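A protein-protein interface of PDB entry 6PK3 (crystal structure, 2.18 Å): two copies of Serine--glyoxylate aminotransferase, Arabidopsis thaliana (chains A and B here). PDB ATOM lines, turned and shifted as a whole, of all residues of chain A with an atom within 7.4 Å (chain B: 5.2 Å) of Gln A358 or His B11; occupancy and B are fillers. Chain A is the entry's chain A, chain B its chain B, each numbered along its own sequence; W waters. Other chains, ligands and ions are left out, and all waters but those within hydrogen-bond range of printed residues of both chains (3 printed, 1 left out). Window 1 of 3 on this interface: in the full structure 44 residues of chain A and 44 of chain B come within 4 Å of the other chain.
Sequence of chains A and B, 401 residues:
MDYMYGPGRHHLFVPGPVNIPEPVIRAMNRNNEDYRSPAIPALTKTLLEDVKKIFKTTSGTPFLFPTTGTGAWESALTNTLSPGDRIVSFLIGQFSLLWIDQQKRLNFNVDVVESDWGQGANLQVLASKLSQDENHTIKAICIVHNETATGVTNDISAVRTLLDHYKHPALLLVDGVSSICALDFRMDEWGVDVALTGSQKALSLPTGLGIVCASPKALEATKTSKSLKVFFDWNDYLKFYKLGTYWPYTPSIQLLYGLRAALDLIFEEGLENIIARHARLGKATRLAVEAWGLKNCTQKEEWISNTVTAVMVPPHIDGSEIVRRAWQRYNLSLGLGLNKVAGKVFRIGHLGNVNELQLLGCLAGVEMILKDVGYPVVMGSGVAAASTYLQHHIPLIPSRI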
ATOM      1  N   ARG A   9      35.095  27.933 -10.983  1.00  0.00           N
ATOM      2  CA  ARG A   9      34.948  28.013  -9.538  1.00  0.00           C
ATOM      3  C   ARG A   9      35.486  26.742  -8.894  1.00  0.00           C
ATOM      4  O   ARG A   9      35.208  25.632  -9.360  1.00  0.00           O
ATOM      5  CB  ARG A   9      33.478  28.218  -9.163  1.00  0.00           C
ATOM      6  CG  ARG A   9      33.269  28.990  -7.863  1.00  0.00           C
ATOM      7  CD  ARG A   9      31.957  29.774  -7.878  1.00  0.00           C
ATOM      8  NE  ARG A   9      31.870  30.674  -9.028  1.00  0.00           N
ATOM      9  CZ  ARG A   9      32.211  31.961  -9.020  1.00  0.00           C
ATOM     10  NH1 ARG A   9      32.665  32.538  -7.914  1.00  0.00           N
ATOM     11  NH2 ARG A   9      32.092  32.677 -10.129  1.00  0.00           N
ATOM     12  N   HIS A  10      36.266  26.909  -7.830  1.00  0.00           N
ATOM     13  CA  HIS A  10      36.785  25.762  -7.101  1.00  0.00           C
ATOM     14  C   HIS A  10      35.644  24.996  -6.444  1.00  0.00           C
ATOM     15  O   HIS A  10      34.705  25.588  -5.906  1.00  0.00           O
ATOM     16  CB  HIS A  10      37.790  26.215  -6.044  1.00  0.00           C
ATOM     17  CG  HIS A  10      38.292  25.101  -5.181  1.00  0.00           C
ATOM     18  ND1 HIS A  10      39.090  24.088  -5.664  1.00  0.00           N
ATOM     19  CD2 HIS A  10      38.101  24.836  -3.867  1.00  0.00           C
ATOM     20  CE1 HIS A  10      39.374  23.249  -4.685  1.00  0.00           C
ATOM     21  NE2 HIS A  10      38.788  23.681  -3.583  1.00  0.00           N
ATOM     22  N   HIS A  11      35.732  23.669  -6.485  1.00  0.00           N
ATOM     23  CA  HIS A  11      34.703  22.796  -5.925  1.00  0.00           C
ATOM     24  C   HIS A  11      35.180  22.322  -4.558  1.00  0.00           C
ATOM     25  O   HIS A  11      35.998  21.404  -4.447  1.00  0.00           O
ATOM     26  CB  HIS A  11      34.409  21.647  -6.879  1.00  0.00           C
ATOM     27  CG  HIS A  11      33.866  22.105  -8.194  1.00  0.00           C
ATOM     28  ND1 HIS A  11      32.516  22.250  -8.429  1.00  0.00           N
ATOM     29  CD2 HIS A  11      34.491  22.488  -9.331  1.00  0.00           C
ATOM     30  CE1 HIS A  11      32.332  22.686  -9.663  1.00  0.00           C
ATOM     31  NE2 HIS A  11      33.515  22.838 -10.232  1.00  0.00           N
ATOM     32  N   LEU A  12      34.655  22.963  -3.518  1.00  0.00           N
ATOM     33  CA  LEU A  12      35.105  22.778  -2.142  1.00  0.00           C
ATOM     34  C   LEU A  12      34.184  21.768  -1.471  1.00  0.00           C
ATOM     35  O   LEU A  12      33.068  22.100  -1.068  1.00  0.00           O
ATOM     36  CB  LEU A  12      35.100  24.117  -1.413  1.00  0.00           C
ATOM     37  CG  LEU A  12      35.589  24.159   0.032  1.00  0.00           C
ATOM     38  CD1 LEU A  12      37.088  23.909   0.106  1.00  0.00           C
ATOM     39  CD2 LEU A  12      35.228  25.500   0.651  1.00  0.00           C
ATOM     40  N   PHE A  13      34.656  20.532  -1.343  1.00  0.00           N
ATOM     41  CA  PHE A  13      33.852  19.457  -0.776  1.00  0.00           C
ATOM     42  C   PHE A  13      34.614  18.727   0.316  1.00  0.00           C
ATOM     43  O   PHE A  13      34.498  17.509   0.482  1.00  0.00           O
ATOM     44  CB  PHE A  13      33.382  18.507  -1.872  1.00  0.00           C
ATOM     45  CG  PHE A  13      32.233  19.055  -2.666  1.00  0.00           C
ATOM     46  CD1 PHE A  13      32.459  19.873  -3.759  1.00  0.00           C
ATOM     47  CD2 PHE A  13      30.928  18.793  -2.288  1.00  0.00           C
ATOM     48  CE1 PHE A  13      31.408  20.394  -4.475  1.00  0.00           C
ATOM     49  CE2 PHE A  13      29.871  19.314  -3.001  1.00  0.00           C
ATOM     50  CZ  PHE A  13      30.111  20.115  -4.096  1.00  0.00           C
ATOM     51  N   ASN A  19      31.642  26.168   2.032  1.00  0.00           N
ATOM     52  CA  ASN A  19      31.357  27.313   1.180  1.00  0.00           C
ATOM     53  C   ASN A  19      30.645  28.407   1.967  1.00  0.00           C
ATOM     54  O   ASN A  19      29.744  28.139   2.765  1.00  0.00           O
ATOM     55  CB  ASN A  19      30.498  26.887  -0.010  1.00  0.00           C
ATOM     56  CG  ASN A  19      31.219  25.922  -0.936  1.00  0.00           C
ATOM     57  OD1 ASN A  19      31.062  24.703  -0.833  1.00  0.00           O
ATOM     58  ND2 ASN A  19      32.019  26.468  -1.846  1.00  0.00           N
ATOM     59  N   LEU A 281      21.236  15.427   0.796  1.00  0.00           N
ATOM     60  CA  LEU A 281      22.575  15.365   0.222  1.00  0.00           C
ATOM     61  C   LEU A 281      23.328  14.136   0.709  1.00  0.00           C
ATOM     62  O   LEU A 281      24.031  13.480  -0.070  1.00  0.00           O
ATOM     63  CB  LEU A 281      23.352  16.633   0.574  1.00  0.00           C
ATOM     64  CG  LEU A 281      22.717  17.950   0.119  1.00  0.00           C
ATOM     65  CD1 LEU A 281      23.478  19.133   0.707  1.00  0.00           C
ATOM     66  CD2 LEU A 281      22.677  18.035  -1.397  1.00  0.00           C
ATOM     67  N   LEU A 332      38.955  20.309  -7.573  1.00  0.00           N
ATOM     68  CA  LEU A 332      38.027  19.760  -6.597  1.00  0.00           C
ATOM     69  C   LEU A 332      38.794  19.418  -5.329  1.00  0.00           C
ATOM     70  O   LEU A 332      39.875  18.821  -5.396  1.00  0.00           O
ATOM     71  CB  LEU A 332      37.321  18.519  -7.160  1.00  0.00           C
ATOM     72  CG  LEU A 332      36.521  17.635  -6.203  1.00  0.00           C
ATOM     73  CD1 LEU A 332      35.333  18.385  -5.618  1.00  0.00           C
ATOM     74  CD2 LEU A 332      36.058  16.374  -6.918  1.00  0.00           C
ATOM     75  N   ASN A 353      26.338  25.538   3.205  1.00  0.00           N
ATOM     76  CA  ASN A 353      25.568  26.166   2.134  1.00  0.00           C
ATOM     77  C   ASN A 353      25.974  25.539   0.807  1.00  0.00           C
ATOM     78  O   ASN A 353      26.895  25.997   0.129  1.00  0.00           O
ATOM     79  CB  ASN A 353      25.792  27.673   2.131  1.00  0.00           C
ATOM     80  CG  ASN A 353      24.965  28.381   1.078  1.00  0.00           C
ATOM     81  OD1 ASN A 353      23.753  28.522   1.224  1.00  0.00           O
ATOM     82  ND2 ASN A 353      25.619  28.836   0.014  1.00  0.00           N
ATOM     83  N   VAL A 354      25.269  24.476   0.433  1.00  0.00           N
ATOM     84  CA  VAL A 354      25.523  23.758  -0.811  1.00  0.00           C
ATOM     85  C   VAL A 354      24.210  23.135  -1.262  1.00  0.00           C
ATOM     86  O   VAL A 354      23.427  22.650  -0.441  1.00  0.00           O
ATOM     87  CB  VAL A 354      26.632  22.699  -0.629  1.00  0.00           C
ATOM     88  CG1 VAL A 354      26.246  21.700   0.453  1.00  0.00           C
ATOM     89  CG2 VAL A 354      26.916  21.987  -1.938  1.00  0.00           C
ATOM     90  N   ASN A 355      23.959  23.167  -2.568  1.00  0.00           N
ATOM     91  CA  ASN A 355      22.721  22.656  -3.143  1.00  0.00           C
ATOM     92  C   ASN A 355      23.002  21.406  -3.976  1.00  0.00           C
ATOM     93  O   ASN A 355      24.145  20.962  -4.117  1.00  0.00           O
ATOM     94  CB  ASN A 355      22.022  23.738  -3.971  1.00  0.00           C
ATOM     95  CG  ASN A 355      22.889  24.284  -5.090  1.00  0.00           C
ATOM     96  OD1 ASN A 355      23.601  23.541  -5.769  1.00  0.00           O
ATOM     97  ND2 ASN A 355      22.829  25.594  -5.289  1.00  0.00           N
ATOM     98  N   GLU A 356      21.930  20.848  -4.548  1.00  0.00           N
ATOM     99  CA  GLU A 356      22.001  19.524  -5.163  1.00  0.00           C
ATOM    100  C   GLU A 356      22.895  19.505  -6.398  1.00  0.00           C
ATOM    101  O   GLU A 356      23.670  18.561  -6.591  1.00  0.00           O
ATOM    102  CB  GLU A 356      20.597  19.045  -5.526  1.00  0.00           C
ATOM    103  CG  GLU A 356      19.752  18.608  -4.339  1.00  0.00           C
ATOM    104  CD  GLU A 356      19.177  19.771  -3.545  1.00  0.00           C
ATOM    105  OE1 GLU A 356      19.383  20.939  -3.940  1.00  0.00           O
ATOM    106  OE2 GLU A 356      18.507  19.514  -2.522  1.00  0.00           O
ATOM    107  N   LEU A 357      22.785  20.512  -7.268  1.00  0.00           N
ATOM    108  CA  LEU A 357      23.591  20.500  -8.485  1.00  0.00           C
ATOM    109  C   LEU A 357      25.078  20.627  -8.178  1.00  0.00           C
ATOM    110  O   LEU A 357      25.907  20.071  -8.908  1.00  0.00           O
ATOM    111  CB  LEU A 357      23.154  21.620  -9.431  1.00  0.00           C
ATOM    112  CG  LEU A 357      21.709  21.616  -9.938  1.00  0.00           C
ATOM    113  CD1 LEU A 357      21.614  22.394 -11.246  1.00  0.00           C
ATOM    114  CD2 LEU A 357      21.165  20.222 -10.106  1.00  0.00           C
ATOM    115  N   GLN A 358      25.439  21.359  -7.123  1.00  0.00           N
ATOM    116  CA  GLN A 358      26.838  21.399  -6.704  1.00  0.00           C
ATOM    117  C   GLN A 358      27.335  20.001  -6.360  1.00  0.00           C
ATOM    118  O   GLN A 358      28.415  19.586  -6.799  1.00  0.00           O
ATOM    119  CB  GLN A 358      27.007  22.335  -5.508  1.00  0.00           C
ATOM    120  CG  GLN A 358      26.894  23.810  -5.841  1.00  0.00           C
ATOM    121  CD  GLN A 358      27.022  24.689  -4.614  1.00  0.00           C
ATOM    122  OE1 GLN A 358      26.041  24.954  -3.921  1.00  0.00           O
ATOM    123  NE2 GLN A 358      28.235  25.143  -4.339  1.00  0.00           N
ATOM    124  N   LEU A 359      26.548  19.256  -5.581  1.00  0.00           N
ATOM    125  CA  LEU A 359      26.950  17.908  -5.195  1.00  0.00           C
ATOM    126  C   LEU A 359      27.070  17.007  -6.417  1.00  0.00           C
ATOM    127  O   LEU A 359      28.042  16.257  -6.556  1.00  0.00           O
ATOM    128  CB  LEU A 359      25.948  17.330  -4.196  1.00  0.00           C
ATOM    129  CG  LEU A 359      26.193  15.886  -3.749  1.00  0.00           C
ATOM    130  CD1 LEU A 359      27.400  15.796  -2.820  1.00  0.00           C
ATOM    131  CD2 LEU A 359      24.958  15.319  -3.073  1.00  0.00           C
ATOM    132  N   LEU A 360      26.083  17.066  -7.315  1.00  0.00           N
ATOM    133  CA  LEU A 360      26.119  16.214  -8.500  1.00  0.00           C
ATOM    134  C   LEU A 360      27.356  16.495  -9.342  1.00  0.00           C
ATOM    135  O   LEU A 360      27.928  15.579  -9.942  1.00  0.00           O
ATOM    136  CB  LEU A 360      24.844  16.405  -9.321  1.00  0.00           C
ATOM    137  CG  LEU A 360      23.587  15.840  -8.657  1.00  0.00           C
ATOM    138  CD1 LEU A 360      22.337  16.346  -9.343  1.00  0.00           C
ATOM    139  CD2 LEU A 360      23.614  14.319  -8.665  1.00  0.00           C
ATOM    140  N   GLY A 361      27.790  17.755  -9.399  1.00  0.00           N
ATOM    141  CA  GLY A 361      29.047  18.053 -10.063  1.00  0.00           C
ATOM    142  C   GLY A 361      30.217  17.348  -9.408  1.00  0.00           C
ATOM    143  O   GLY A 361      31.073  16.775 -10.087  1.00  0.00           O
ATOM    144  N   CYS A 362      30.265  17.372  -8.076  1.00  0.00           N
ATOM    145  CA  CYS A 362      31.318  16.660  -7.362  1.00  0.00           C
ATOM    146  C   CYS A 362      31.266  15.167  -7.663  1.00  0.00           C
ATOM    147  O   CYS A 362      32.291  14.548  -7.972  1.00  0.00           O
ATOM    148  CB  CYS A 362      31.185  16.917  -5.862  1.00  0.00           C
ATOM    149  SG  CYS A 362      32.234  15.876  -4.837  1.00  0.00           S
ATOM    150  N   LEU A 363      30.070  14.574  -7.600  1.00  0.00           N
ATOM    151  CA  LEU A 363      29.947  13.134  -7.797  1.00  0.00           C
ATOM    152  C   LEU A 363      30.359  12.731  -9.206  1.00  0.00           C
ATOM    153  O   LEU A 363      31.016  11.699  -9.398  1.00  0.00           O
ATOM    154  CB  LEU A 363      28.514  12.684  -7.514  1.00  0.00           C
ATOM    155  CG  LEU A 363      27.997  12.960  -6.102  1.00  0.00           C
ATOM    156  CD1 LEU A 363      26.561  12.472  -5.961  1.00  0.00           C
ATOM    157  CD2 LEU A 363      28.892  12.313  -5.059  1.00  0.00           C
ATOM    158  N   ALA A 364      29.972  13.524 -10.209  1.00  0.00           N
ATOM    159  CA  ALA A 364      30.411  13.252 -11.573  1.00  0.00           C
ATOM    160  C   ALA A 364      31.929  13.303 -11.674  1.00  0.00           C
ATOM    161  O   ALA A 364      32.540  12.498 -12.386  1.00  0.00           O
ATOM    162  CB  ALA A 364      29.776  14.248 -12.543  1.00  0.00           C
ATOM    163  N   GLY B   8      22.667  27.287  -1.490  1.00  0.00           N
ATOM    164  CA  GLY B   8      23.812  26.973  -2.322  1.00  0.00           C
ATOM    165  C   GLY B   8      24.103  28.080  -3.322  1.00  0.00           C
ATOM    166  O   GLY B   8      23.469  29.132  -3.344  1.00  0.00           O
ATOM    167  N   ARG B   9      25.092  27.821  -4.173  1.00  0.00           N
ATOM    168  CA  ARG B   9      25.477  28.792  -5.186  1.00  0.00           C
ATOM    169  C   ARG B   9      24.573  28.679  -6.405  1.00  0.00           C
ATOM    170  O   ARG B   9      24.263  27.579  -6.872  1.00  0.00           O
ATOM    171  CB  ARG B   9      26.937  28.601  -5.597  1.00  0.00           C
ATOM    172  CG  ARG B   9      27.916  29.433  -4.770  1.00  0.00           C
ATOM    173  CD  ARG B   9      29.239  29.674  -5.497  1.00  0.00           C
ATOM    174  NE  ARG B   9      30.346  28.929  -4.898  1.00  0.00           N
ATOM    175  CZ  ARG B   9      30.843  27.787  -5.370  1.00  0.00           C
ATOM    176  NH1 ARG B   9      30.349  27.227  -6.468  1.00  0.00           N
ATOM    177  NH2 ARG B   9      31.851  27.202  -4.736  1.00  0.00           N
ATOM    178  N   HIS B  10      24.142  29.833  -6.911  1.00  0.00           N
ATOM    179  CA  HIS B  10      23.329  29.868  -8.117  1.00  0.00           C
ATOM    180  C   HIS B  10      24.146  29.402  -9.314  1.00  0.00           C
ATOM    181  O   HIS B  10      25.302  29.794  -9.490  1.00  0.00           O
ATOM    182  CB  HIS B  10      22.801  31.280  -8.362  1.00  0.00           C
ATOM    183  CG  HIS B  10      22.025  31.424  -9.635  1.00  0.00           C
ATOM    184  ND1 HIS B  10      20.745  30.939  -9.785  1.00  0.00           N
ATOM    185  CD2 HIS B  10      22.350  31.999 -10.817  1.00  0.00           C
ATOM    186  CE1 HIS B  10      20.312  31.211 -11.004  1.00  0.00           C
ATOM    187  NE2 HIS B  10      21.267  31.853 -11.650  1.00  0.00           N
ATOM    188  N   HIS B  11      23.536  28.561 -10.141  1.00  0.00           N
ATOM    189  CA  HIS B  11      24.190  28.007 -11.322  1.00  0.00           C
ATOM    190  C   HIS B  11      23.803  28.859 -12.523  1.00  0.00           C
ATOM    191  O   HIS B  11      22.693  28.754 -13.050  1.00  0.00           O
ATOM    192  CB  HIS B  11      23.804  26.544 -11.491  1.00  0.00           C
ATOM    193  CG  HIS B  11      24.149  25.705 -10.302  1.00  0.00           C
ATOM    194  ND1 HIS B  11      25.341  25.022 -10.195  1.00  0.00           N
ATOM    195  CD2 HIS B  11      23.474  25.466  -9.154  1.00  0.00           C
ATOM    196  CE1 HIS B  11      25.377  24.382  -9.039  1.00  0.00           C
ATOM    197  NE2 HIS B  11      24.257  24.636  -8.388  1.00  0.00           N
ATOM    198  N   LEU B  12      24.734  29.709 -12.952  1.00  0.00           N
ATOM    199  CA  LEU B  12      24.493  30.683 -14.015  1.00  0.00           C
ATOM    200  C   LEU B  12      24.941  30.074 -15.338  1.00  0.00           C
ATOM    201  O   LEU B  12      26.136  30.025 -15.640  1.00  0.00           O
ATOM    202  CB  LEU B  12      25.233  31.979 -13.715  1.00  0.00           C
ATOM    203  CG  LEU B  12      24.940  33.186 -14.607  1.00  0.00           C
ATOM    204  CD1 LEU B  12      23.542  33.737 -14.361  1.00  0.00           C
ATOM    205  CD2 LEU B  12      25.997  34.261 -14.374  1.00  0.00           C
ATOM    206  N   PHE B  13      23.983  29.611 -16.135  1.00  0.00           N
ATOM    207  CA  PHE B  13      24.281  28.984 -17.417  1.00  0.00           C
ATOM    208  C   PHE B  13      23.444  29.595 -18.530  1.00  0.00           C
ATOM    209  O   PHE B  13      22.978  28.906 -19.442  1.00  0.00           O
ATOM    210  CB  PHE B  13      24.097  27.471 -17.332  1.00  0.00           C
ATOM    211  CG  PHE B  13      25.245  26.778 -16.656  1.00  0.00           C
ATOM    212  CD1 PHE B  13      25.284  26.658 -15.276  1.00  0.00           C
ATOM    213  CD2 PHE B  13      26.307  26.289 -17.396  1.00  0.00           C
ATOM    214  CE1 PHE B  13      26.347  26.043 -14.650  1.00  0.00           C
ATOM    215  CE2 PHE B  13      27.374  25.674 -16.778  1.00  0.00           C
ATOM    216  CZ  PHE B  13      27.395  25.552 -15.399  1.00  0.00           C
ATOM    217  N   TYR B 330      15.802  24.256  -8.867  1.00  0.00           N
ATOM    218  CA  TYR B 330      17.193  23.829  -8.916  1.00  0.00           C
ATOM    219  C   TYR B 330      18.189  24.973  -8.814  1.00  0.00           C
ATOM    220  O   TYR B 330      19.398  24.726  -8.898  1.00  0.00           O
ATOM    221  CB  TYR B 330      17.452  23.047 -10.212  1.00  0.00           C
ATOM    222  CG  TYR B 330      16.569  21.828 -10.347  1.00  0.00           C
ATOM    223  CD1 TYR B 330      16.888  20.645  -9.697  1.00  0.00           C
ATOM    224  CD2 TYR B 330      15.409  21.866 -11.108  1.00  0.00           C
ATOM    225  CE1 TYR B 330      16.084  19.531  -9.807  1.00  0.00           C
ATOM    226  CE2 TYR B 330      14.593  20.750 -11.222  1.00  0.00           C
ATOM    227  CZ  TYR B 330      14.939  19.586 -10.568  1.00  0.00           C
ATOM    228  OH  TYR B 330      14.142  18.473 -10.671  1.00  0.00           O
ATOM    229  N   ASN B 331      17.729  26.208  -8.625  1.00  0.00           N
ATOM    230  CA  ASN B 331      18.615  27.365  -8.542  1.00  0.00           C
ATOM    231  C   ASN B 331      19.554  27.403  -9.746  1.00  0.00           C
ATOM    232  O   ASN B 331      20.770  27.563  -9.622  1.00  0.00           O
ATOM    233  CB  ASN B 331      19.396  27.358  -7.229  1.00  0.00           C
ATOM    234  CG  ASN B 331      19.862  28.741  -6.823  1.00  0.00           C
ATOM    235  OD1 ASN B 331      19.631  29.720  -7.535  1.00  0.00           O
ATOM    236  ND2 ASN B 331      20.509  28.832  -5.667  1.00  0.00           N
ATOM    237  N   LEU B 332      18.966  27.249 -10.929  1.00  0.00           N
ATOM    238  CA  LEU B 332      19.705  27.145 -12.180  1.00  0.00           C
ATOM    239  C   LEU B 332      19.102  28.114 -13.184  1.00  0.00           C
ATOM    240  O   LEU B 332      17.876  28.195 -13.317  1.00  0.00           O
ATOM    241  CB  LEU B 332      19.666  25.710 -12.721  1.00  0.00           C
ATOM    242  CG  LEU B 332      20.124  25.462 -14.159  1.00  0.00           C
ATOM    243  CD1 LEU B 332      21.615  25.713 -14.326  1.00  0.00           C
ATOM    244  CD2 LEU B 332      19.772  24.044 -14.576  1.00  0.00           C
ATOM    245  N   SER B 333      19.964  28.849 -13.878  1.00  0.00           N
ATOM    246  CA  SER B 333      19.558  29.806 -14.898  1.00  0.00           C
ATOM    247  C   SER B 333      19.938  29.257 -16.265  1.00  0.00           C
ATOM    248  O   SER B 333      21.123  29.056 -16.549  1.00  0.00           O
ATOM    249  CB  SER B 333      20.215  31.165 -14.659  1.00  0.00           C
ATOM    250  OG  SER B 333      19.412  31.965 -13.816  1.00  0.00           O
HETATM  251  O   HOH W   1      34.960  27.748  -4.066  1.00  0.00           O
HETATM  252  O   HOH W   2      20.442  22.938  -7.068  1.00  0.00           O
HETATM  253  O   HOH W   3      30.636  23.961  -5.987  1.00  0.00           O
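NE2 of His B11 sits at hydrogen-bond distance from OD1 of Asn A355.
OD1 of Asn A353 sits at hydrogen-bond distance from N of Gly B8.
The backbone carbonyl oxygen of His A10 is in hydrogen-bond range of the guanidinium group of Arg B9 (3.5 Å).
The backbone carbonyl oxygen (O) of Arg B9 lies within hydrogen-bond range of the side-chain amide nitrogen (ND2) of Asn A355 (2.9 Å).
N of Arg B9 lies within hydrogen-bond range of OE1 of Gln A358 (3.0 Å).
The guanidinium group (NH2) of Arg B9 lies close to the side-chain amide nitrogen (ND2) of Asn A19.
OD1 of Asn A19 lies close to O of Leu A12 (3.3 Å).
The backbone carbonyl oxygen (O) of Arg A9 sits close to a ring nitrogen (NE2) of His A11 (3.4 Å).
OD1 of Asn A355 sits close to N of Leu A357 (3.5 Å).
A ring nitrogen (NE2) of His B11 sits close to the backbone carbonyl oxygen (O) of Arg B9 (3.3 Å).
The side-chain amide oxygen (OE1) of Gln A358 sits at hydrogen-bond distance from the backbone NH (N) of Asn A355 (3.1 Å).
The backbone NH (N) of Ser B333 is in hydrogen-bond range of the backbone carbonyl oxygen (O) of His B11 (2.9 Å).
Among the printed residues, pairs that only touch across the chains: Arg A9 with Arg B9 (3.3 Å), Leu A357 with His B11 (3.4 Å), Gln A358 with Gly B8 (3.4 Å), Asn A355 with Gly B8 (3.4 Å), Gln A358 with His B11 (3.6 Å), Val A354 with Gly B8 (3.9 Å) and Leu A357 with Tyr B330 (3.98 Å).
Printed residues of chain B within 4 Å of Asn A19: Arg B9.
Of the printed residues of chain B, Asn A355 touches Gly B8 (3.4 Å), Arg B9 (2.9 Å) and His B11 (2.9 Å).
Of the printed residues of chain B, Leu A357 touches His B11 and Tyr B330.
Gly A361 touches none of the printed residues of chain B.
Printed residues of chain A within 4 Å of Gly B8: Asn A353, Val A354, Asn A355 and Gln A358.
Of chain A, only Asn A355 (2.9 Å), Leu A357 (3.4 Å) and Gln A358 (3.6 Å) come within 4 Å of His B11.
Printed residues of chain A within 4 Å of Tyr B330: Leu A357.
The nearest residue of chain A that does not touch His B11 is Glu A356 (5.7 Å).
The nearest printed residue of chain B that does not touch Leu A357 is Leu B332 (4.1 Å).
Printed residues of chain B that touch a printed residue of chain A: Gly B8, Arg B9, His B11 and Tyr B330.
Hydrophobic or aromatic side chains of chain A that line the printed part of chain B: Leu A357.
Arg B9 touches its own counterpart, Arg A9.
His A10 touches Arg B9, but with the chains exchanged Arg A9 does not touch His B10 (6.6 Å).
6 positions are printed for both chains.
Of the 13 pairs that touch across the chains among the printed residues, 1 has its exchanged pair printed and touching as well.
Water W2 lies within hydrogen-bond range of O of Tyr B330 (2.8 Å), N of Leu A357 (3.4 Å) and OD1 of Asn A355 (3.5 Å).
Water W1 bridges O of His A10 (2.8 Å) and NH2 of Arg B9 (3.2 Å).
Water W3 bridges NE2 of Gln A358 (3.1 Å) and NH1 of Arg B9 (3.3 Å).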
